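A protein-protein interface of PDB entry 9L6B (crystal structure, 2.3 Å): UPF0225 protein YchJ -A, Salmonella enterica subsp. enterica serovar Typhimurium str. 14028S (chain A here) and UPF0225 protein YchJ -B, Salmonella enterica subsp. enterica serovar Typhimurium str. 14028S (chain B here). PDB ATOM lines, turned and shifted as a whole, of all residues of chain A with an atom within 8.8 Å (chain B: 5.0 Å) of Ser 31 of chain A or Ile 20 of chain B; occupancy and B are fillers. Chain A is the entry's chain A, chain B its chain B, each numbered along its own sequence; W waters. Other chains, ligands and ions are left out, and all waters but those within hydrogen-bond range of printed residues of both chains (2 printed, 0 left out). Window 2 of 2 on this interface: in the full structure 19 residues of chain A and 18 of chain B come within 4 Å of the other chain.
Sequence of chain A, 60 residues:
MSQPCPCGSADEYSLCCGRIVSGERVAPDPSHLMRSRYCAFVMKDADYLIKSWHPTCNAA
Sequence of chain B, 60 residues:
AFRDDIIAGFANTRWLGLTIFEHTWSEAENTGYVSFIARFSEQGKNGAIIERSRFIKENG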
ATOM      1  N   CYS A   7      -0.922   1.127  31.647  1.00  0.00           N
ATOM      2  CA  CYS A   7      -0.722  -0.122  30.882  1.00  0.00           C
ATOM      3  C   CYS A   7      -2.146  -0.532  30.506  1.00  0.00           C
ATOM      4  O   CYS A   7      -2.438  -0.882  29.358  1.00  0.00           O
ATOM      5  CB  CYS A   7       0.062  -1.311  31.667  1.00  0.00           C
ATOM      6  SG  CYS A   7       1.662  -1.100  32.855  1.00  0.00           S
ATOM      7  N   GLY A   8      -3.066  -0.408  31.456  1.00  0.00           N
ATOM      8  CA  GLY A   8      -4.320  -1.128  31.407  1.00  0.00           C
ATOM      9  C   GLY A   8      -4.251  -2.493  32.059  1.00  0.00           C
ATOM     10  O   GLY A   8      -5.213  -3.270  31.955  1.00  0.00           O
ATOM     11  N   CYS A  16       3.951  -2.153  37.644  1.00  0.00           N
ATOM     12  CA  CYS A  16       3.768  -2.552  36.247  1.00  0.00           C
ATOM     13  C   CYS A  16       4.799  -1.808  35.409  1.00  0.00           C
ATOM     14  O   CYS A  16       5.995  -2.085  35.490  1.00  0.00           O
ATOM     15  CB  CYS A  16       2.326  -2.250  35.753  1.00  0.00           C
ATOM     16  SG  CYS A  16       1.811  -2.789  34.040  1.00  0.00           S
ATOM     17  N   CYS A  17       4.346  -0.814  34.655  1.00  0.00           N
ATOM     18  CA  CYS A  17       5.230  -0.104  33.743  1.00  0.00           C
ATOM     19  C   CYS A  17       6.230   0.808  34.463  1.00  0.00           C
ATOM     20  O   CYS A  17       7.287   1.116  33.902  1.00  0.00           O
ATOM     21  CB  CYS A  17       4.352   0.661  32.750  1.00  0.00           C
ATOM     22  SG  CYS A  17       3.307  -0.494  31.804  1.00  0.00           S
ATOM     23  N   ILE A  20       9.868  -0.342  34.902  1.00  0.00           N
ATOM     24  CA  ILE A  20      10.650  -0.339  33.672  1.00  0.00           C
ATOM     25  C   ILE A  20      11.053   1.082  33.310  1.00  0.00           C
ATOM     26  O   ILE A  20      12.202   1.345  32.942  1.00  0.00           O
ATOM     27  CB  ILE A  20       9.855  -1.021  32.545  1.00  0.00           C
ATOM     28  CG1 ILE A  20       9.689  -2.510  32.883  1.00  0.00           C
ATOM     29  CG2 ILE A  20      10.556  -0.822  31.212  1.00  0.00           C
ATOM     30  CD1 ILE A  20       8.813  -3.300  31.932  1.00  0.00           C
ATOM     31  N   ALA A  27      12.884  -4.647  30.689  1.00  0.00           N
ATOM     32  CA  ALA A  27      11.638  -5.148  30.128  1.00  0.00           C
ATOM     33  C   ALA A  27      11.836  -6.554  29.592  1.00  0.00           C
ATOM     34  O   ALA A  27      12.645  -6.747  28.677  1.00  0.00           O
ATOM     35  CB  ALA A  27      11.148  -4.230  29.020  1.00  0.00           C
ATOM     36  N   PRO A  28      11.113  -7.559  30.098  1.00  0.00           N
ATOM     37  CA  PRO A  28      11.415  -8.951  29.724  1.00  0.00           C
ATOM     38  C   PRO A  28      11.006  -9.330  28.317  1.00  0.00           C
ATOM     39  O   PRO A  28      11.542 -10.315  27.806  1.00  0.00           O
ATOM     40  CB  PRO A  28      10.632  -9.777  30.752  1.00  0.00           C
ATOM     41  CG  PRO A  28       9.528  -8.870  31.211  1.00  0.00           C
ATOM     42  CD  PRO A  28      10.076  -7.467  31.142  1.00  0.00           C
ATOM     43  N   ASP A  29      10.088  -8.620  27.663  1.00  0.00           N
ATOM     44  CA  ASP A  29       9.659  -9.042  26.337  1.00  0.00           C
ATOM     45  C   ASP A  29       9.114  -7.824  25.600  1.00  0.00           C
ATOM     46  O   ASP A  29       8.966  -6.754  26.194  1.00  0.00           O
ATOM     47  CB  ASP A  29       8.620 -10.182  26.421  1.00  0.00           C
ATOM     48  CG  ASP A  29       7.366  -9.793  27.178  1.00  0.00           C
ATOM     49  OD1 ASP A  29       6.881  -8.651  27.024  1.00  0.00           O
ATOM     50  OD2 ASP A  29       6.833 -10.671  27.890  1.00  0.00           O
ATOM     51  N   PRO A  30       8.811  -7.946  24.305  1.00  0.00           N
ATOM     52  CA  PRO A  30       8.305  -6.754  23.585  1.00  0.00           C
ATOM     53  C   PRO A  30       6.961  -6.255  24.101  1.00  0.00           C
ATOM     54  O   PRO A  30       6.718  -5.042  24.091  1.00  0.00           O
ATOM     55  CB  PRO A  30       8.226  -7.207  22.114  1.00  0.00           C
ATOM     56  CG  PRO A  30       8.584  -8.657  22.081  1.00  0.00           C
ATOM     57  CD  PRO A  30       9.209  -9.036  23.390  1.00  0.00           C
ATOM     58  N   SER A  31       6.086  -7.144  24.570  1.00  0.00           N
ATOM     59  CA  SER A  31       4.804  -6.700  25.109  1.00  0.00           C
ATOM     60  C   SER A  31       4.995  -5.748  26.284  1.00  0.00           C
ATOM     61  O   SER A  31       4.375  -4.687  26.343  1.00  0.00           O
ATOM     62  CB  SER A  31       3.984  -7.911  25.534  1.00  0.00           C
ATOM     63  OG  SER A  31       2.737  -7.498  26.022  1.00  0.00           O
ATOM     64  N   HIS A  32       5.860  -6.109  27.231  1.00  0.00           N
ATOM     65  CA  HIS A  32       6.130  -5.215  28.346  1.00  0.00           C
ATOM     66  C   HIS A  32       6.756  -3.914  27.873  1.00  0.00           C
ATOM     67  O   HIS A  32       6.495  -2.854  28.450  1.00  0.00           O
ATOM     68  CB  HIS A  32       7.038  -5.895  29.378  1.00  0.00           C
ATOM     69  CG  HIS A  32       6.393  -7.048  30.098  1.00  0.00           C
ATOM     70  ND1 HIS A  32       6.481  -7.214  31.467  1.00  0.00           N
ATOM     71  CD2 HIS A  32       5.657  -8.094  29.641  1.00  0.00           C
ATOM     72  CE1 HIS A  32       5.818  -8.304  31.821  1.00  0.00           C
ATOM     73  NE2 HIS A  32       5.305  -8.854  30.732  1.00  0.00           N
ATOM     74  N   LEU A  33       7.615  -3.966  26.847  1.00  0.00           N
ATOM     75  CA  LEU A  33       8.233  -2.730  26.366  1.00  0.00           C
ATOM     76  C   LEU A  33       7.188  -1.819  25.748  1.00  0.00           C
ATOM     77  O   LEU A  33       7.183  -0.608  25.998  1.00  0.00           O
ATOM     78  CB  LEU A  33       9.335  -3.023  25.335  1.00  0.00           C
ATOM     79  CG  LEU A  33      10.249  -1.823  25.048  1.00  0.00           C
ATOM     80  CD1 LEU A  33      11.216  -1.615  26.234  1.00  0.00           C
ATOM     81  CD2 LEU A  33      11.037  -1.957  23.739  1.00  0.00           C
ATOM     82  N   MET A  34       6.319  -2.393  24.919  1.00  0.00           N
ATOM     83  CA  MET A  34       5.234  -1.641  24.303  1.00  0.00           C
ATOM     84  C   MET A  34       4.388  -0.953  25.359  1.00  0.00           C
ATOM     85  O   MET A  34       4.148   0.251  25.284  1.00  0.00           O
ATOM     86  CB  MET A  34       4.369  -2.578  23.458  1.00  0.00           C
ATOM     87  CG  MET A  34       3.167  -1.874  22.834  1.00  0.00           C
ATOM     88  SD  MET A  34       3.744  -0.564  21.721  1.00  0.00           S
ATOM     89  CE  MET A  34       2.504   0.701  22.061  1.00  0.00           C
ATOM     90  N   ARG A  35       3.951  -1.706  26.367  1.00  0.00           N
ATOM     91  CA  ARG A  35       3.184  -1.108  27.453  1.00  0.00           C
ATOM     92  C   ARG A  35       3.930   0.050  28.073  1.00  0.00           C
ATOM     93  O   ARG A  35       3.347   1.116  28.301  1.00  0.00           O
ATOM     94  CB  ARG A  35       2.868  -2.155  28.523  1.00  0.00           C
ATOM     95  CG  ARG A  35       1.641  -2.941  28.197  1.00  0.00           C
ATOM     96  CD  ARG A  35       1.414  -4.036  29.242  1.00  0.00           C
ATOM     97  NE  ARG A  35       0.567  -5.098  28.721  1.00  0.00           N
ATOM     98  CZ  ARG A  35      -0.749  -5.182  28.902  1.00  0.00           C
ATOM     99  NH1 ARG A  35      -1.426  -4.238  29.550  1.00  0.00           N
ATOM    100  NH2 ARG A  35      -1.407  -6.239  28.415  1.00  0.00           N
ATOM    101  N   SER A  36       5.226  -0.130  28.343  1.00  0.00           N
ATOM    102  CA  SER A  36       5.970   0.910  29.051  1.00  0.00           C
ATOM    103  C   SER A  36       6.174   2.151  28.189  1.00  0.00           C
ATOM    104  O   SER A  36       6.262   3.262  28.722  1.00  0.00           O
ATOM    105  CB  SER A  36       7.317   0.371  29.523  1.00  0.00           C
ATOM    106  OG  SER A  36       8.205   0.238  28.421  1.00  0.00           O
ATOM    107  N   ARG A  37       6.279   2.001  26.868  1.00  0.00           N
ATOM    108  CA  ARG A  37       6.375   3.196  26.028  1.00  0.00           C
ATOM    109  C   ARG A  37       5.029   3.899  25.917  1.00  0.00           C
ATOM    110  O   ARG A  37       4.981   5.127  25.828  1.00  0.00           O
ATOM    111  CB  ARG A  37       6.889   2.844  24.623  1.00  0.00           C
ATOM    112  CG  ARG A  37       8.346   2.329  24.558  1.00  0.00           C
ATOM    113  CD  ARG A  37       8.725   1.885  23.138  1.00  0.00           C
ATOM    114  NE  ARG A  37       8.563   2.923  22.123  1.00  0.00           N
ATOM    115  CZ  ARG A  37       9.470   3.851  21.860  1.00  0.00           C
ATOM    116  NH1 ARG A  37      10.598   3.929  22.545  1.00  0.00           N
ATOM    117  NH2 ARG A  37       9.236   4.734  20.891  1.00  0.00           N
ATOM    118  N   TYR A  38       3.928   3.145  25.891  1.00  0.00           N
ATOM    119  CA  TYR A  38       2.621   3.787  25.933  1.00  0.00           C
ATOM    120  C   TYR A  38       2.477   4.618  27.205  1.00  0.00           C
ATOM    121  O   TYR A  38       1.996   5.754  27.161  1.00  0.00           O
ATOM    122  CB  TYR A  38       1.518   2.733  25.832  1.00  0.00           C
ATOM    123  CG  TYR A  38       0.131   3.318  26.053  1.00  0.00           C
ATOM    124  CD1 TYR A  38      -0.571   3.924  25.005  1.00  0.00           C
ATOM    125  CD2 TYR A  38      -0.466   3.291  27.313  1.00  0.00           C
ATOM    126  CE1 TYR A  38      -1.828   4.474  25.207  1.00  0.00           C
ATOM    127  CE2 TYR A  38      -1.742   3.841  27.522  1.00  0.00           C
ATOM    128  CZ  TYR A  38      -2.412   4.430  26.469  1.00  0.00           C
ATOM    129  OH  TYR A  38      -3.670   4.981  26.662  1.00  0.00           O
ATOM    130  N   LEU B  18      -5.106   1.420  25.861  1.00  0.00           N
ATOM    131  CA  LEU B  18      -4.247   0.512  25.112  1.00  0.00           C
ATOM    132  C   LEU B  18      -4.795  -0.902  25.211  1.00  0.00           C
ATOM    133  O   LEU B  18      -4.998  -1.420  26.312  1.00  0.00           O
ATOM    134  CB  LEU B  18      -2.814   0.546  25.637  1.00  0.00           C
ATOM    135  CG  LEU B  18      -1.855  -0.426  24.928  1.00  0.00           C
ATOM    136  CD1 LEU B  18      -1.619   0.005  23.479  1.00  0.00           C
ATOM    137  CD2 LEU B  18      -0.536  -0.567  25.678  1.00  0.00           C
ATOM    138  N   THR B  19      -5.026  -1.523  24.062  1.00  0.00           N
ATOM    139  CA  THR B  19      -5.487  -2.904  23.989  1.00  0.00           C
ATOM    140  C   THR B  19      -4.519  -3.696  23.121  1.00  0.00           C
ATOM    141  O   THR B  19      -4.344  -3.392  21.936  1.00  0.00           O
ATOM    142  CB  THR B  19      -6.907  -2.968  23.419  1.00  0.00           C
ATOM    143  OG1 THR B  19      -7.724  -2.019  24.110  1.00  0.00           O
ATOM    144  CG2 THR B  19      -7.505  -4.346  23.593  1.00  0.00           C
ATOM    145  N   ILE B  20      -3.897  -4.708  23.693  1.00  0.00           N
ATOM    146  CA  ILE B  20      -2.975  -5.558  22.952  1.00  0.00           C
ATOM    147  C   ILE B  20      -3.732  -6.806  22.534  1.00  0.00           C
ATOM    148  O   ILE B  20      -4.412  -7.435  23.353  1.00  0.00           O
ATOM    149  CB  ILE B  20      -1.731  -5.865  23.796  1.00  0.00           C
ATOM    150  CG1 ILE B  20      -0.863  -4.597  23.835  1.00  0.00           C
ATOM    151  CG2 ILE B  20      -0.980  -7.064  23.246  1.00  0.00           C
ATOM    152  CD1 ILE B  20       0.362  -4.672  24.740  1.00  0.00           C
ATOM    153  N   PHE B  21      -3.695  -7.122  21.245  1.00  0.00           N
ATOM    154  CA  PHE B  21      -4.453  -8.260  20.761  1.00  0.00           C
ATOM    155  C   PHE B  21      -3.612  -9.283  20.018  1.00  0.00           C
ATOM    156  O   PHE B  21      -4.173 -10.272  19.555  1.00  0.00           O
ATOM    157  CB  PHE B  21      -5.630  -7.801  19.874  1.00  0.00           C
ATOM    158  CG  PHE B  21      -5.228  -7.000  18.656  1.00  0.00           C
ATOM    159  CD1 PHE B  21      -5.045  -5.638  18.736  1.00  0.00           C
ATOM    160  CD2 PHE B  21      -5.062  -7.615  17.428  1.00  0.00           C
ATOM    161  CE1 PHE B  21      -4.693  -4.903  17.611  1.00  0.00           C
ATOM    162  CE2 PHE B  21      -4.709  -6.889  16.304  1.00  0.00           C
ATOM    163  CZ  PHE B  21      -4.527  -5.535  16.390  1.00  0.00           C
ATOM    164  N   GLU B  22      -2.301  -9.077  19.889  1.00  0.00           N
ATOM    165  CA  GLU B  22      -1.392 -10.076  19.332  1.00  0.00           C
ATOM    166  C   GLU B  22       0.033  -9.741  19.759  1.00  0.00           C
ATOM    167  O   GLU B  22       0.400  -8.567  19.873  1.00  0.00           O
ATOM    168  CB  GLU B  22      -1.481 -10.154  17.803  1.00  0.00           C
ATOM    169  CG  GLU B  22      -0.522 -11.167  17.146  1.00  0.00           C
ATOM    170  CD  GLU B  22       0.825 -10.554  16.713  1.00  0.00           C
ATOM    171  OE1 GLU B  22       0.986  -9.311  16.740  1.00  0.00           O
ATOM    172  OE2 GLU B  22       1.737 -11.321  16.352  1.00  0.00           O
ATOM    173  N   HIS B  23       0.835 -10.793  19.958  1.00  0.00           N
ATOM    174  CA  HIS B  23       2.205 -10.666  20.449  1.00  0.00           C
ATOM    175  C   HIS B  23       2.985 -11.926  20.085  1.00  0.00           C
ATOM    176  O   HIS B  23       2.515 -13.035  20.355  1.00  0.00           O
ATOM    177  CB  HIS B  23       2.191 -10.443  21.973  1.00  0.00           C
ATOM    178  CG  HIS B  23       3.550 -10.369  22.601  1.00  0.00           C
ATOM    179  ND1 HIS B  23       3.819 -10.903  23.847  1.00  0.00           N
ATOM    180  CD2 HIS B  23       4.709  -9.812  22.174  1.00  0.00           C
ATOM    181  CE1 HIS B  23       5.083 -10.686  24.152  1.00  0.00           C
ATOM    182  NE2 HIS B  23       5.641 -10.014  23.160  1.00  0.00           N
ATOM    183  N   VAL B  34       4.171  -6.557  18.390  1.00  0.00           N
ATOM    184  CA  VAL B  34       3.050  -6.299  19.294  1.00  0.00           C
ATOM    185  C   VAL B  34       1.996  -5.564  18.479  1.00  0.00           C
ATOM    186  O   VAL B  34       2.251  -4.456  17.992  1.00  0.00           O
ATOM    187  CB  VAL B  34       3.455  -5.463  20.522  1.00  0.00           C
ATOM    188  CG1 VAL B  34       2.266  -5.251  21.433  1.00  0.00           C
ATOM    189  CG2 VAL B  34       4.589  -6.114  21.303  1.00  0.00           C
ATOM    190  N   SER B  35       0.827  -6.170  18.313  1.00  0.00           N
ATOM    191  CA  SER B  35      -0.295  -5.523  17.650  1.00  0.00           C
ATOM    192  C   SER B  35      -1.203  -4.891  18.689  1.00  0.00           C
ATOM    193  O   SER B  35      -1.506  -5.515  19.711  1.00  0.00           O
ATOM    194  CB  SER B  35      -1.098  -6.528  16.822  1.00  0.00           C
ATOM    195  OG  SER B  35      -0.319  -7.084  15.780  1.00  0.00           O
ATOM    196  N   PHE B  36      -1.670  -3.670  18.420  1.00  0.00           N
ATOM    197  CA  PHE B  36      -2.407  -2.976  19.469  1.00  0.00           C
ATOM    198  C   PHE B  36      -3.340  -1.906  18.898  1.00  0.00           C
ATOM    199  O   PHE B  36      -3.163  -1.406  17.778  1.00  0.00           O
ATOM    200  CB  PHE B  36      -1.439  -2.364  20.495  1.00  0.00           C
ATOM    201  CG  PHE B  36      -0.584  -1.254  19.940  1.00  0.00           C
ATOM    202  CD1 PHE B  36       0.677  -1.521  19.423  1.00  0.00           C
ATOM    203  CD2 PHE B  36      -1.051   0.061  19.922  1.00  0.00           C
ATOM    204  CE1 PHE B  36       1.467  -0.493  18.892  1.00  0.00           C
ATOM    205  CE2 PHE B  36      -0.270   1.089  19.405  1.00  0.00           C
ATOM    206  CZ  PHE B  36       0.983   0.821  18.885  1.00  0.00           C
HETATM  207  O   HOH W   1      -3.946  -5.097  26.701  1.00  0.00           O
HETATM  208  O   HOH W   2      -4.991   1.098  28.678  1.00  0.00           O
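The side-chain carboxylate of Asp 29 of chain A sits at hydrogen-bond distance from the backbone NH of His 32 of chain A (2.7 Å). The side-chain sulfur (SG) of Cys 16 of chain A is disulfide-bonded to the side-chain sulfur (SG) of Cys 7 of chain A, 2.1 Å away. SG of Cys 7 of chain A is disulfide-bonded to SG of Cys 17 of chain A (2.0 Å). N of Ser 31 of chain A sits at hydrogen-bond distance from OD1 of Asp 29 of chain A (3.0 Å).
Among the printed residues, pairs that only touch across the chains: Asp 29 of chain A with His 23 of chain B, Pro 30 of chain A with His 23 of chain B, Pro 30 of chain A with Val 34 of chain B, Ser 31 of chain A with Ile 20 of chain B, Ser 31 of chain A with Val 34 of chain B, Met 34 of chain A with Val 34 of chain B, Met 34 of chain A with Phe 36 of chain B and Tyr 38 of chain A with Leu 18 of chain B.
Pro 28 of chain A touches none of the printed residues of chain B. Of the printed residues of chain B, Asp 29 of chain A touches His 23. Ser 31 of chain A touches just these residues of chain B: Ile 20, His 23 and Val 34. Of the printed residues of chain B, Met 34 of chain A touches Val 34 and Phe 36. Printed residues of chain B within 4 Å of Tyr 38 of chain A: Leu 18. Printed residues of chain A within 4 Å of Ile 20 of chain B: Ser 31 (3.9 Å). Glu 22 of chain B touches none of the printed residues of chain A. Of the printed residues of chain A, Phe 36 of chain B touches Met 34. The nearest printed residue of chain B that does not touch Asp 29 of chain A is Val 34 of chain B (6.5 Å).
Printed residues of chain B that touch a printed residue of chain A: Leu 18, Ile 20, His 23, Val 34 and Phe 36. Hydrophobic or aromatic side chains of chain B within 4 Å of the printed part of chain A: Leu 18, Ile 20, His 23, Val 34 and Phe 36. Of the 17 printed residues of chain A, 5 touch a printed residue of chain B. Printed residues of chain A that touch a printed residue of chain B: Asp 29, Pro 30, Ser 31, Met 34 and Tyr 38. Hydrophobic or aromatic side chains of chain A within 4 Å of the printed part of chain B: Pro 30, Met 34 and Tyr 38.
Water W2 lies within hydrogen-bond range of N of Leu 18 of chain B and O of Cys 7 of chain A. Water W1 lies within hydrogen-bond range of N of Ile 20 of chain B (3.0 Å) and NH2 of Arg 35 of chain A (3.3 Å).
The backbone NH (N) of Ser 31 of chain A sits at hydrogen-bond distance from a ring nitrogen (NE2) of His 23 of chain B (3.2 Å).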
